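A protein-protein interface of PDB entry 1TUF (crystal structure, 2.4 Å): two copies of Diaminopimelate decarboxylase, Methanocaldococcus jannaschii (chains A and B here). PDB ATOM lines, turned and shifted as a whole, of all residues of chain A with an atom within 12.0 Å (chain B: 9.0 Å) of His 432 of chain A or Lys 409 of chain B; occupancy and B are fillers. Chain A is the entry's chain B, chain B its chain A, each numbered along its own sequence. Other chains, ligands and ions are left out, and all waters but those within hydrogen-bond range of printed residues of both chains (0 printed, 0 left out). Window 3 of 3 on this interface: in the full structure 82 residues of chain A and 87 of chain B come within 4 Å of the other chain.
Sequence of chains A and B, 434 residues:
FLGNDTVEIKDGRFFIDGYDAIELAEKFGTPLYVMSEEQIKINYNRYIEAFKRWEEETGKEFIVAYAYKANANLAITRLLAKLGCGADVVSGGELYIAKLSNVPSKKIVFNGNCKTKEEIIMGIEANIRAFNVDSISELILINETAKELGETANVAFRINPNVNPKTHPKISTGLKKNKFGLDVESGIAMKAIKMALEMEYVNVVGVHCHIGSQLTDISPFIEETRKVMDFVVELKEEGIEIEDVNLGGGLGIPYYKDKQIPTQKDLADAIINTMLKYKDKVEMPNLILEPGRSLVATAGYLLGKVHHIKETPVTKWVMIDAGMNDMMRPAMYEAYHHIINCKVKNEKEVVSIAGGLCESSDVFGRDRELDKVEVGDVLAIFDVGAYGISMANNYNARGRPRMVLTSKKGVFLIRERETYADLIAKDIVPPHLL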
ATOM      1  N   ILE A 428     -21.012 -26.783 -10.805  1.00  0.00           N
ATOM      2  CA  ILE A 428     -21.038 -25.814  -9.720  1.00  0.00           C
ATOM      3  C   ILE A 428     -19.638 -25.510  -9.198  1.00  0.00           C
ATOM      4  O   ILE A 428     -18.915 -26.406  -8.765  1.00  0.00           O
ATOM      5  CB  ILE A 428     -21.944 -26.312  -8.573  1.00  0.00           C
ATOM      6  CG1 ILE A 428     -23.382 -26.455  -9.094  1.00  0.00           C
ATOM      7  CG2 ILE A 428     -21.915 -25.323  -7.417  1.00  0.00           C
ATOM      8  CD1 ILE A 428     -24.338 -27.113  -8.120  1.00  0.00           C
ATOM      9  N   VAL A 429     -19.253 -24.239  -9.256  1.00  0.00           N
ATOM     10  CA  VAL A 429     -17.930 -23.819  -8.807  1.00  0.00           C
ATOM     11  C   VAL A 429     -17.897 -23.552  -7.301  1.00  0.00           C
ATOM     12  O   VAL A 429     -18.683 -22.764  -6.780  1.00  0.00           O
ATOM     13  CB  VAL A 429     -17.478 -22.537  -9.528  1.00  0.00           C
ATOM     14  CG1 VAL A 429     -16.092 -22.114  -9.021  1.00  0.00           C
ATOM     15  CG2 VAL A 429     -17.453 -22.766 -11.012  1.00  0.00           C
ATOM     16  N   PRO A 430     -16.983 -24.217  -6.579  1.00  0.00           N
ATOM     17  CA  PRO A 430     -16.880 -24.022  -5.129  1.00  0.00           C
ATOM     18  C   PRO A 430     -16.385 -22.614  -4.788  1.00  0.00           C
ATOM     19  O   PRO A 430     -15.690 -21.976  -5.583  1.00  0.00           O
ATOM     20  CB  PRO A 430     -15.893 -25.110  -4.701  1.00  0.00           C
ATOM     21  CG  PRO A 430     -16.093 -26.177  -5.747  1.00  0.00           C
ATOM     22  CD  PRO A 430     -16.153 -25.353  -7.010  1.00  0.00           C
ATOM     23  N   PRO A 431     -16.729 -22.117  -3.592  1.00  0.00           N
ATOM     24  CA  PRO A 431     -16.316 -20.775  -3.164  1.00  0.00           C
ATOM     25  C   PRO A 431     -14.845 -20.416  -3.420  1.00  0.00           C
ATOM     26  O   PRO A 431     -14.555 -19.393  -4.045  1.00  0.00           O
ATOM     27  CB  PRO A 431     -16.664 -20.763  -1.675  1.00  0.00           C
ATOM     28  CG  PRO A 431     -17.825 -21.720  -1.581  1.00  0.00           C
ATOM     29  CD  PRO A 431     -17.413 -22.837  -2.500  1.00  0.00           C
ATOM     30  N   HIS A 432     -13.911 -21.243  -2.955  1.00  0.00           N
ATOM     31  CA  HIS A 432     -12.503 -20.908  -3.154  1.00  0.00           C
ATOM     32  C   HIS A 432     -12.087 -20.877  -4.615  1.00  0.00           C
ATOM     33  O   HIS A 432     -10.948 -20.537  -4.920  1.00  0.00           O
ATOM     34  CB  HIS A 432     -11.572 -21.851  -2.368  1.00  0.00           C
ATOM     35  CG  HIS A 432     -11.449 -23.224  -2.950  1.00  0.00           C
ATOM     36  ND1 HIS A 432     -12.345 -24.235  -2.679  1.00  0.00           N
ATOM     37  CD2 HIS A 432     -10.539 -23.748  -3.807  1.00  0.00           C
ATOM     38  CE1 HIS A 432     -11.995 -25.321  -3.346  1.00  0.00           C
ATOM     39  NE2 HIS A 432     -10.902 -25.052  -4.038  1.00  0.00           N
ATOM     40  N   LEU A 433     -12.993 -21.216  -5.527  1.00  0.00           N
ATOM     41  CA  LEU A 433     -12.631 -21.185  -6.941  1.00  0.00           C
ATOM     42  C   LEU A 433     -13.371 -20.120  -7.740  1.00  0.00           C
ATOM     43  O   LEU A 433     -13.140 -19.969  -8.938  1.00  0.00           O
ATOM     44  CB  LEU A 433     -12.834 -22.558  -7.582  1.00  0.00           C
ATOM     45  CG  LEU A 433     -11.928 -23.682  -7.064  1.00  0.00           C
ATOM     46  CD1 LEU A 433     -12.224 -24.987  -7.812  1.00  0.00           C
ATOM     47  CD2 LEU A 433     -10.471 -23.285  -7.257  1.00  0.00           C
ATOM     48  N   LEU A 434     -14.259 -19.381  -7.083  1.00  0.00           N
ATOM     49  CA  LEU A 434     -15.005 -18.323  -7.758  1.00  0.00           C
ATOM     50  C   LEU A 434     -14.025 -17.252  -8.187  1.00  0.00           C
ATOM     51  O   LEU A 434     -13.173 -16.856  -7.397  1.00  0.00           O
ATOM     52  CB  LEU A 434     -16.035 -17.710  -6.813  1.00  0.00           C
ATOM     53  CG  LEU A 434     -17.175 -18.664  -6.453  1.00  0.00           C
ATOM     54  CD1 LEU A 434     -17.901 -18.174  -5.205  1.00  0.00           C
ATOM     55  CD2 LEU A 434     -18.113 -18.780  -7.647  1.00  0.00           C
ATOM     56  N   ASP B  17      -7.343 -37.793  -0.648  1.00  0.00           N
ATOM     57  CA  ASP B  17      -7.063 -36.502  -0.015  1.00  0.00           C
ATOM     58  C   ASP B  17      -7.525 -36.528   1.445  1.00  0.00           C
ATOM     59  O   ASP B  17      -8.105 -35.561   1.936  1.00  0.00           O
ATOM     60  CB  ASP B  17      -7.782 -35.361  -0.738  1.00  0.00           C
ATOM     61  CG  ASP B  17      -7.236 -35.108  -2.129  1.00  0.00           C
ATOM     62  OD1 ASP B  17      -6.000 -35.113  -2.296  1.00  0.00           O
ATOM     63  OD2 ASP B  17      -8.045 -34.888  -3.056  1.00  0.00           O
ATOM     64  N   TYR B  19      -9.956 -38.059   2.771  1.00  0.00           N
ATOM     65  CA  TYR B  19     -11.373 -38.353   2.919  1.00  0.00           C
ATOM     66  C   TYR B  19     -11.671 -39.830   2.712  1.00  0.00           C
ATOM     67  O   TYR B  19     -11.106 -40.476   1.827  1.00  0.00           O
ATOM     68  CB  TYR B  19     -12.184 -37.507   1.932  1.00  0.00           C
ATOM     69  CG  TYR B  19     -12.046 -36.022   2.171  1.00  0.00           C
ATOM     70  CD1 TYR B  19     -12.750 -35.391   3.204  1.00  0.00           C
ATOM     71  CD2 TYR B  19     -11.189 -35.250   1.384  1.00  0.00           C
ATOM     72  CE1 TYR B  19     -12.605 -34.019   3.450  1.00  0.00           C
ATOM     73  CE2 TYR B  19     -11.032 -33.887   1.615  1.00  0.00           C
ATOM     74  CZ  TYR B  19     -11.742 -33.270   2.649  1.00  0.00           C
ATOM     75  OH  TYR B  19     -11.587 -31.911   2.860  1.00  0.00           O
ATOM     76  N   GLU B  37      -8.350 -32.213  -6.013  1.00  0.00           N
ATOM     77  CA  GLU B  37      -7.783 -30.913  -6.335  1.00  0.00           C
ATOM     78  C   GLU B  37      -6.248 -30.965  -6.286  1.00  0.00           C
ATOM     79  O   GLU B  37      -5.569 -30.520  -7.218  1.00  0.00           O
ATOM     80  CB  GLU B  37      -8.331 -29.870  -5.362  1.00  0.00           C
ATOM     81  CG  GLU B  37      -7.814 -28.470  -5.592  1.00  0.00           C
ATOM     82  CD  GLU B  37      -8.589 -27.443  -4.799  1.00  0.00           C
ATOM     83  OE1 GLU B  37      -9.754 -27.171  -5.156  1.00  0.00           O
ATOM     84  OE2 GLU B  37      -8.041 -26.914  -3.806  1.00  0.00           O
ATOM     85  N   GLU B  38      -5.709 -31.519  -5.201  1.00  0.00           N
ATOM     86  CA  GLU B  38      -4.262 -31.643  -5.035  1.00  0.00           C
ATOM     87  C   GLU B  38      -3.598 -32.426  -6.159  1.00  0.00           C
ATOM     88  O   GLU B  38      -2.569 -31.998  -6.693  1.00  0.00           O
ATOM     89  CB  GLU B  38      -3.928 -32.298  -3.685  1.00  0.00           C
ATOM     90  CG  GLU B  38      -3.940 -31.316  -2.529  1.00  0.00           C
ATOM     91  CD  GLU B  38      -2.899 -30.223  -2.714  1.00  0.00           C
ATOM     92  OE1 GLU B  38      -3.083 -29.123  -2.150  1.00  0.00           O
ATOM     93  OE2 GLU B  38      -1.893 -30.471  -3.426  1.00  0.00           O
ATOM     94  N   LYS B  41      -2.981 -30.289  -8.934  1.00  0.00           N
ATOM     95  CA  LYS B  41      -1.903 -29.335  -8.689  1.00  0.00           C
ATOM     96  C   LYS B  41      -0.570 -30.034  -8.924  1.00  0.00           C
ATOM     97  O   LYS B  41       0.354 -29.477  -9.529  1.00  0.00           O
ATOM     98  CB  LYS B  41      -1.948 -28.802  -7.251  1.00  0.00           C
ATOM     99  CG  LYS B  41      -3.048 -27.786  -6.970  1.00  0.00           C
ATOM    100  CD  LYS B  41      -2.912 -27.223  -5.552  1.00  0.00           C
ATOM    101  CE  LYS B  41      -4.099 -26.336  -5.160  1.00  0.00           C
ATOM    102  NZ  LYS B  41      -3.962 -25.801  -3.767  1.00  0.00           N
ATOM    103  N   ALA B  75     -15.780 -26.325 -12.477  1.00  0.00           N
ATOM    104  CA  ALA B  75     -14.943 -26.265 -11.290  1.00  0.00           C
ATOM    105  C   ALA B  75     -13.495 -26.658 -11.581  1.00  0.00           C
ATOM    106  O   ALA B  75     -12.566 -26.078 -11.016  1.00  0.00           O
ATOM    107  CB  ALA B  75     -15.515 -27.156 -10.206  1.00  0.00           C
ATOM    108  N   ARG B  78     -11.848 -24.105 -13.890  1.00  0.00           N
ATOM    109  CA  ARG B  78     -11.704 -22.941 -13.033  1.00  0.00           C
ATOM    110  C   ARG B  78     -10.416 -23.100 -12.221  1.00  0.00           C
ATOM    111  O   ARG B  78      -9.586 -22.192 -12.156  1.00  0.00           O
ATOM    112  CB  ARG B  78     -12.906 -22.859 -12.097  1.00  0.00           C
ATOM    113  CG  ARG B  78     -13.114 -21.526 -11.437  1.00  0.00           C
ATOM    114  CD  ARG B  78     -13.812 -20.527 -12.345  1.00  0.00           C
ATOM    115  NE  ARG B  78     -13.927 -19.247 -11.645  1.00  0.00           N
ATOM    116  CZ  ARG B  78     -14.293 -18.100 -12.203  1.00  0.00           C
ATOM    117  NH1 ARG B  78     -14.592 -18.053 -13.494  1.00  0.00           N
ATOM    118  NH2 ARG B  78     -14.344 -16.996 -11.462  1.00  0.00           N
ATOM    119  N   LEU B  79     -10.265 -24.271 -11.612  1.00  0.00           N
ATOM    120  CA  LEU B  79      -9.103 -24.590 -10.796  1.00  0.00           C
ATOM    121  C   LEU B  79      -7.835 -24.499 -11.637  1.00  0.00           C
ATOM    122  O   LEU B  79      -6.866 -23.863 -11.238  1.00  0.00           O
ATOM    123  CB  LEU B  79      -9.265 -25.994 -10.194  1.00  0.00           C
ATOM    124  CG  LEU B  79      -8.164 -26.690  -9.376  1.00  0.00           C
ATOM    125  CD1 LEU B  79      -7.194 -27.325 -10.324  1.00  0.00           C
ATOM    126  CD2 LEU B  79      -7.457 -25.709  -8.423  1.00  0.00           C
ATOM    127  N   LYS B  82      -7.009 -20.890 -12.266  1.00  0.00           N
ATOM    128  CA  LYS B  82      -6.384 -20.243 -11.125  1.00  0.00           C
ATOM    129  C   LYS B  82      -4.893 -20.565 -10.999  1.00  0.00           C
ATOM    130  O   LYS B  82      -4.126 -19.749 -10.501  1.00  0.00           O
ATOM    131  CB  LYS B  82      -7.111 -20.629  -9.839  1.00  0.00           C
ATOM    132  CG  LYS B  82      -8.250 -19.699  -9.470  1.00  0.00           C
ATOM    133  CD  LYS B  82      -8.941 -20.204  -8.211  1.00  0.00           C
ATOM    134  CE  LYS B  82      -9.657 -19.084  -7.472  1.00  0.00           C
ATOM    135  NZ  LYS B  82      -8.707 -18.066  -6.925  1.00  0.00           N
ATOM    136  N   LEU B 405     -15.350 -32.574  -5.523  1.00  0.00           N
ATOM    137  CA  LEU B 405     -13.946 -32.181  -5.558  1.00  0.00           C
ATOM    138  C   LEU B 405     -13.419 -32.224  -4.135  1.00  0.00           C
ATOM    139  O   LEU B 405     -13.960 -31.553  -3.251  1.00  0.00           O
ATOM    140  CB  LEU B 405     -13.790 -30.752  -6.089  1.00  0.00           C
ATOM    141  CG  LEU B 405     -12.354 -30.207  -6.152  1.00  0.00           C
ATOM    142  CD1 LEU B 405     -11.598 -30.945  -7.244  1.00  0.00           C
ATOM    143  CD2 LEU B 405     -12.350 -28.710  -6.438  1.00  0.00           C
ATOM    144  N   THR B 406     -12.381 -33.022  -3.907  1.00  0.00           N
ATOM    145  CA  THR B 406     -11.778 -33.108  -2.583  1.00  0.00           C
ATOM    146  C   THR B 406     -10.562 -32.174  -2.542  1.00  0.00           C
ATOM    147  O   THR B 406      -9.632 -32.330  -3.329  1.00  0.00           O
ATOM    148  CB  THR B 406     -11.330 -34.575  -2.234  1.00  0.00           C
ATOM    149  OG1 THR B 406     -10.476 -35.091  -3.264  1.00  0.00           O
ATOM    150  CG2 THR B 406     -12.538 -35.494  -2.077  1.00  0.00           C
ATOM    151  N   SER B 407     -10.591 -31.186  -1.649  1.00  0.00           N
ATOM    152  CA  SER B 407      -9.479 -30.243  -1.486  1.00  0.00           C
ATOM    153  C   SER B 407      -9.226 -30.028   0.000  1.00  0.00           C
ATOM    154  O   SER B 407      -9.979 -30.522   0.842  1.00  0.00           O
ATOM    155  CB  SER B 407      -9.799 -28.893  -2.139  1.00  0.00           C
ATOM    156  OG  SER B 407     -10.849 -28.225  -1.461  1.00  0.00           O
ATOM    157  N   LYS B 408      -8.172 -29.290   0.329  1.00  0.00           N
ATOM    158  CA  LYS B 408      -7.865 -29.032   1.732  1.00  0.00           C
ATOM    159  C   LYS B 408      -9.002 -28.192   2.304  1.00  0.00           C
ATOM    160  O   LYS B 408      -9.237 -28.177   3.516  1.00  0.00           O
ATOM    161  CB  LYS B 408      -6.533 -28.283   1.875  1.00  0.00           C
ATOM    162  CG  LYS B 408      -5.330 -28.944   1.197  1.00  0.00           C
ATOM    163  CD  LYS B 408      -5.049 -30.369   1.699  1.00  0.00           C
ATOM    164  CE  LYS B 408      -4.404 -30.422   3.103  1.00  0.00           C
ATOM    165  NZ  LYS B 408      -5.275 -29.975   4.241  1.00  0.00           N
ATOM    166  N   LYS B 409      -9.719 -27.504   1.419  1.00  0.00           N
ATOM    167  CA  LYS B 409     -10.838 -26.664   1.837  1.00  0.00           C
ATOM    168  C   LYS B 409     -12.025 -27.528   2.258  1.00  0.00           C
ATOM    169  O   LYS B 409     -12.890 -27.093   3.023  1.00  0.00           O
ATOM    170  CB  LYS B 409     -11.261 -25.731   0.695  1.00  0.00           C
ATOM    171  CG  LYS B 409     -11.011 -24.242   0.944  1.00  0.00           C
ATOM    172  CD  LYS B 409      -9.547 -23.848   0.762  1.00  0.00           C
ATOM    173  CE  LYS B 409      -9.370 -22.313   0.676  1.00  0.00           C
ATOM    174  NZ  LYS B 409      -9.697 -21.569   1.935  1.00  0.00           N
ATOM    175  N   GLY B 410     -12.058 -28.754   1.750  1.00  0.00           N
ATOM    176  CA  GLY B 410     -13.139 -29.667   2.070  1.00  0.00           C
ATOM    177  C   GLY B 410     -13.631 -30.361   0.812  1.00  0.00           C
ATOM    178  O   GLY B 410     -12.989 -30.274  -0.239  1.00  0.00           O
ATOM    179  N   VAL B 411     -14.761 -31.056   0.921  1.00  0.00           N
ATOM    180  CA  VAL B 411     -15.350 -31.756  -0.218  1.00  0.00           C
ATOM    181  C   VAL B 411     -16.528 -30.947  -0.750  1.00  0.00           C
ATOM    182  O   VAL B 411     -17.423 -30.577   0.006  1.00  0.00           O
ATOM    183  CB  VAL B 411     -15.847 -33.174   0.166  1.00  0.00           C
ATOM    184  CG1 VAL B 411     -14.671 -34.105   0.345  1.00  0.00           C
ATOM    185  CG2 VAL B 411     -16.659 -33.119   1.450  1.00  0.00           C
ATOM    186  N   PHE B 412     -16.523 -30.674  -2.052  1.00  0.00           N
ATOM    187  CA  PHE B 412     -17.593 -29.894  -2.658  1.00  0.00           C
ATOM    188  C   PHE B 412     -18.237 -30.572  -3.867  1.00  0.00           C
ATOM    189  O   PHE B 412     -17.560 -31.208  -4.679  1.00  0.00           O
ATOM    190  CB  PHE B 412     -17.055 -28.514  -3.054  1.00  0.00           C
ATOM    191  CG  PHE B 412     -16.353 -27.796  -1.926  1.00  0.00           C
ATOM    192  CD1 PHE B 412     -15.035 -28.109  -1.598  1.00  0.00           C
ATOM    193  CD2 PHE B 412     -17.029 -26.854  -1.148  1.00  0.00           C
ATOM    194  CE1 PHE B 412     -14.405 -27.504  -0.511  1.00  0.00           C
ATOM    195  CE2 PHE B 412     -16.405 -26.246  -0.060  1.00  0.00           C
ATOM    196  CZ  PHE B 412     -15.092 -26.575   0.257  1.00  0.00           C
ATOM    197  N   ILE B 414     -19.219 -30.547  -7.252  1.00  0.00           N
ATOM    198  CA  ILE B 414     -18.916 -29.734  -8.420  1.00  0.00           C
ATOM    199  C   ILE B 414     -19.787 -30.083  -9.623  1.00  0.00           C
ATOM    200  O   ILE B 414     -19.721 -29.427 -10.663  1.00  0.00           O
ATOM    201  CB  ILE B 414     -17.431 -29.871  -8.797  1.00  0.00           C
ATOM    202  CG1 ILE B 414     -17.098 -31.330  -9.099  1.00  0.00           C
ATOM    203  CG2 ILE B 414     -16.569 -29.388  -7.641  1.00  0.00           C
ATOM    204  CD1 ILE B 414     -15.735 -31.518  -9.722  1.00  0.00           C
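Hydrophobic or aromatic side chains of chain B within 4 Å of the printed part of chain A: Ala 75, Leu 79, Leu 405, Phe 412 and Ile 414.
Printed residues of chain A that touch a printed residue of chain B: Ile 428, Val 429, Pro 430, His 432, Leu 433 and Leu 434.
Along chain A the printed residues that touch a printed residue of chain B span positions 428 to 434.
Among the printed residues, 16 pairs touch across the chains.
No position is printed for both chains.
Of the 16 pairs that touch across the chains among the printed residues, none has its exchanged pair printed and touching as well.
Among the printed residues, merely in contact across the chains: Ile 428 of chain A with Ala 75 of chain B (3.8 Å), Val 429 of chain A with Arg 78 of chain B (3.9 Å), Pro 430 of chain A with Ala 75 of chain B (3.7 Å), Pro 430 of chain A with Phe 412 of chain B (3.7 Å), Pro 430 of chain A with Ile 414 of chain B (3.8 Å), His 432 of chain A with Lys 82 of chain B (3.2 Å), His 432 of chain A with Ser 407 of chain B (3.6 Å), His 432 of chain A with Lys 409 of chain B (3.8 Å), Leu 433 of chain A with Ala 75 of chain B (3.4 Å), Leu 433 of chain A with Leu 79 of chain B (3.9 Å), Leu 433 of chain A with Lys 82 of chain B (3.6 Å), Leu 433 of chain A with Leu 405 of chain B (3.97 Å) and Leu 434 of chain A with Arg 78 of chain B (3.3 Å).
The backbone NH of Leu 405 of chain B sits at hydrogen-bond distance from the backbone carbonyl oxygen of Phe 412 of chain B, 2.7 Å away.
The side-chain hydroxyl (OG) of Ser 407 of chain B lies within hydrogen-bond range of the backbone carbonyl oxygen (O) of Gly 410 of chain B (3.2 Å).
The backbone NH of Lys 409 of chain B sits close to the side-chain hydroxyl of Ser 407 of chain B (3.2 Å).
The side-chain hydroxyl (OH) of Tyr 19 of chain B is in hydrogen-bond range of the backbone carbonyl oxygen (O) of Ser 407 of chain B, at 2.9 Å.
The backbone NH (N) of Glu 37 of chain B sits at hydrogen-bond distance from the backbone carbonyl oxygen (O) of Thr 406 of chain B (3.0 Å).
The backbone NH (N) of Ile 428 of chain A is in hydrogen-bond range of the backbone carbonyl oxygen (O) of Ile 414 of chain B (2.9 Å).
NE2 of His 432 of chain A lies within hydrogen-bond range of OE1 of Glu 37 of chain B (2.7 Å).
The guanidinium group of Arg 78 of chain B sits at hydrogen-bond distance from the backbone carbonyl oxygen of Leu 433 of chain A, 2.9 Å away.
Printed residues of chain B within 4 Å of Ile 428 of chain A: Ala 75 and Ile 414.
Printed residues of chain B within 4 Å of Pro 430 of chain A: Ala 75, Phe 412 and Ile 414.
No residue of chain B comes within 4 Å of Pro 431 of chain A.
Leu 433 of chain A touches just these residues of chain B: Ala 75, Arg 78, Leu 79, Lys 82 and Leu 405.
Glu 38 of chain B touches none of the printed residues of chain A.
Lys 41 of chain B touches none of the printed residues of chain A.
Of the printed residues of chain A, Lys 82 of chain B touches His 432 (3.2 Å) and Leu 433 (3.6 Å).
Ser 407 of chain B touches just one residue of chain A: His 432.
Lys 408 of chain B touches none of the printed residues of chain A.
Lys 409 of chain B touches one residue of chain A.
No residue of chain A comes within 4 Å of Gly 410 of chain B.
Of the printed residues of chain A, Ile 414 of chain B touches Ile 428 and Pro 430.
The nearest printed residue of chain A that does not touch Phe 412 of chain B is Pro 431 of chain A (4.3 Å).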
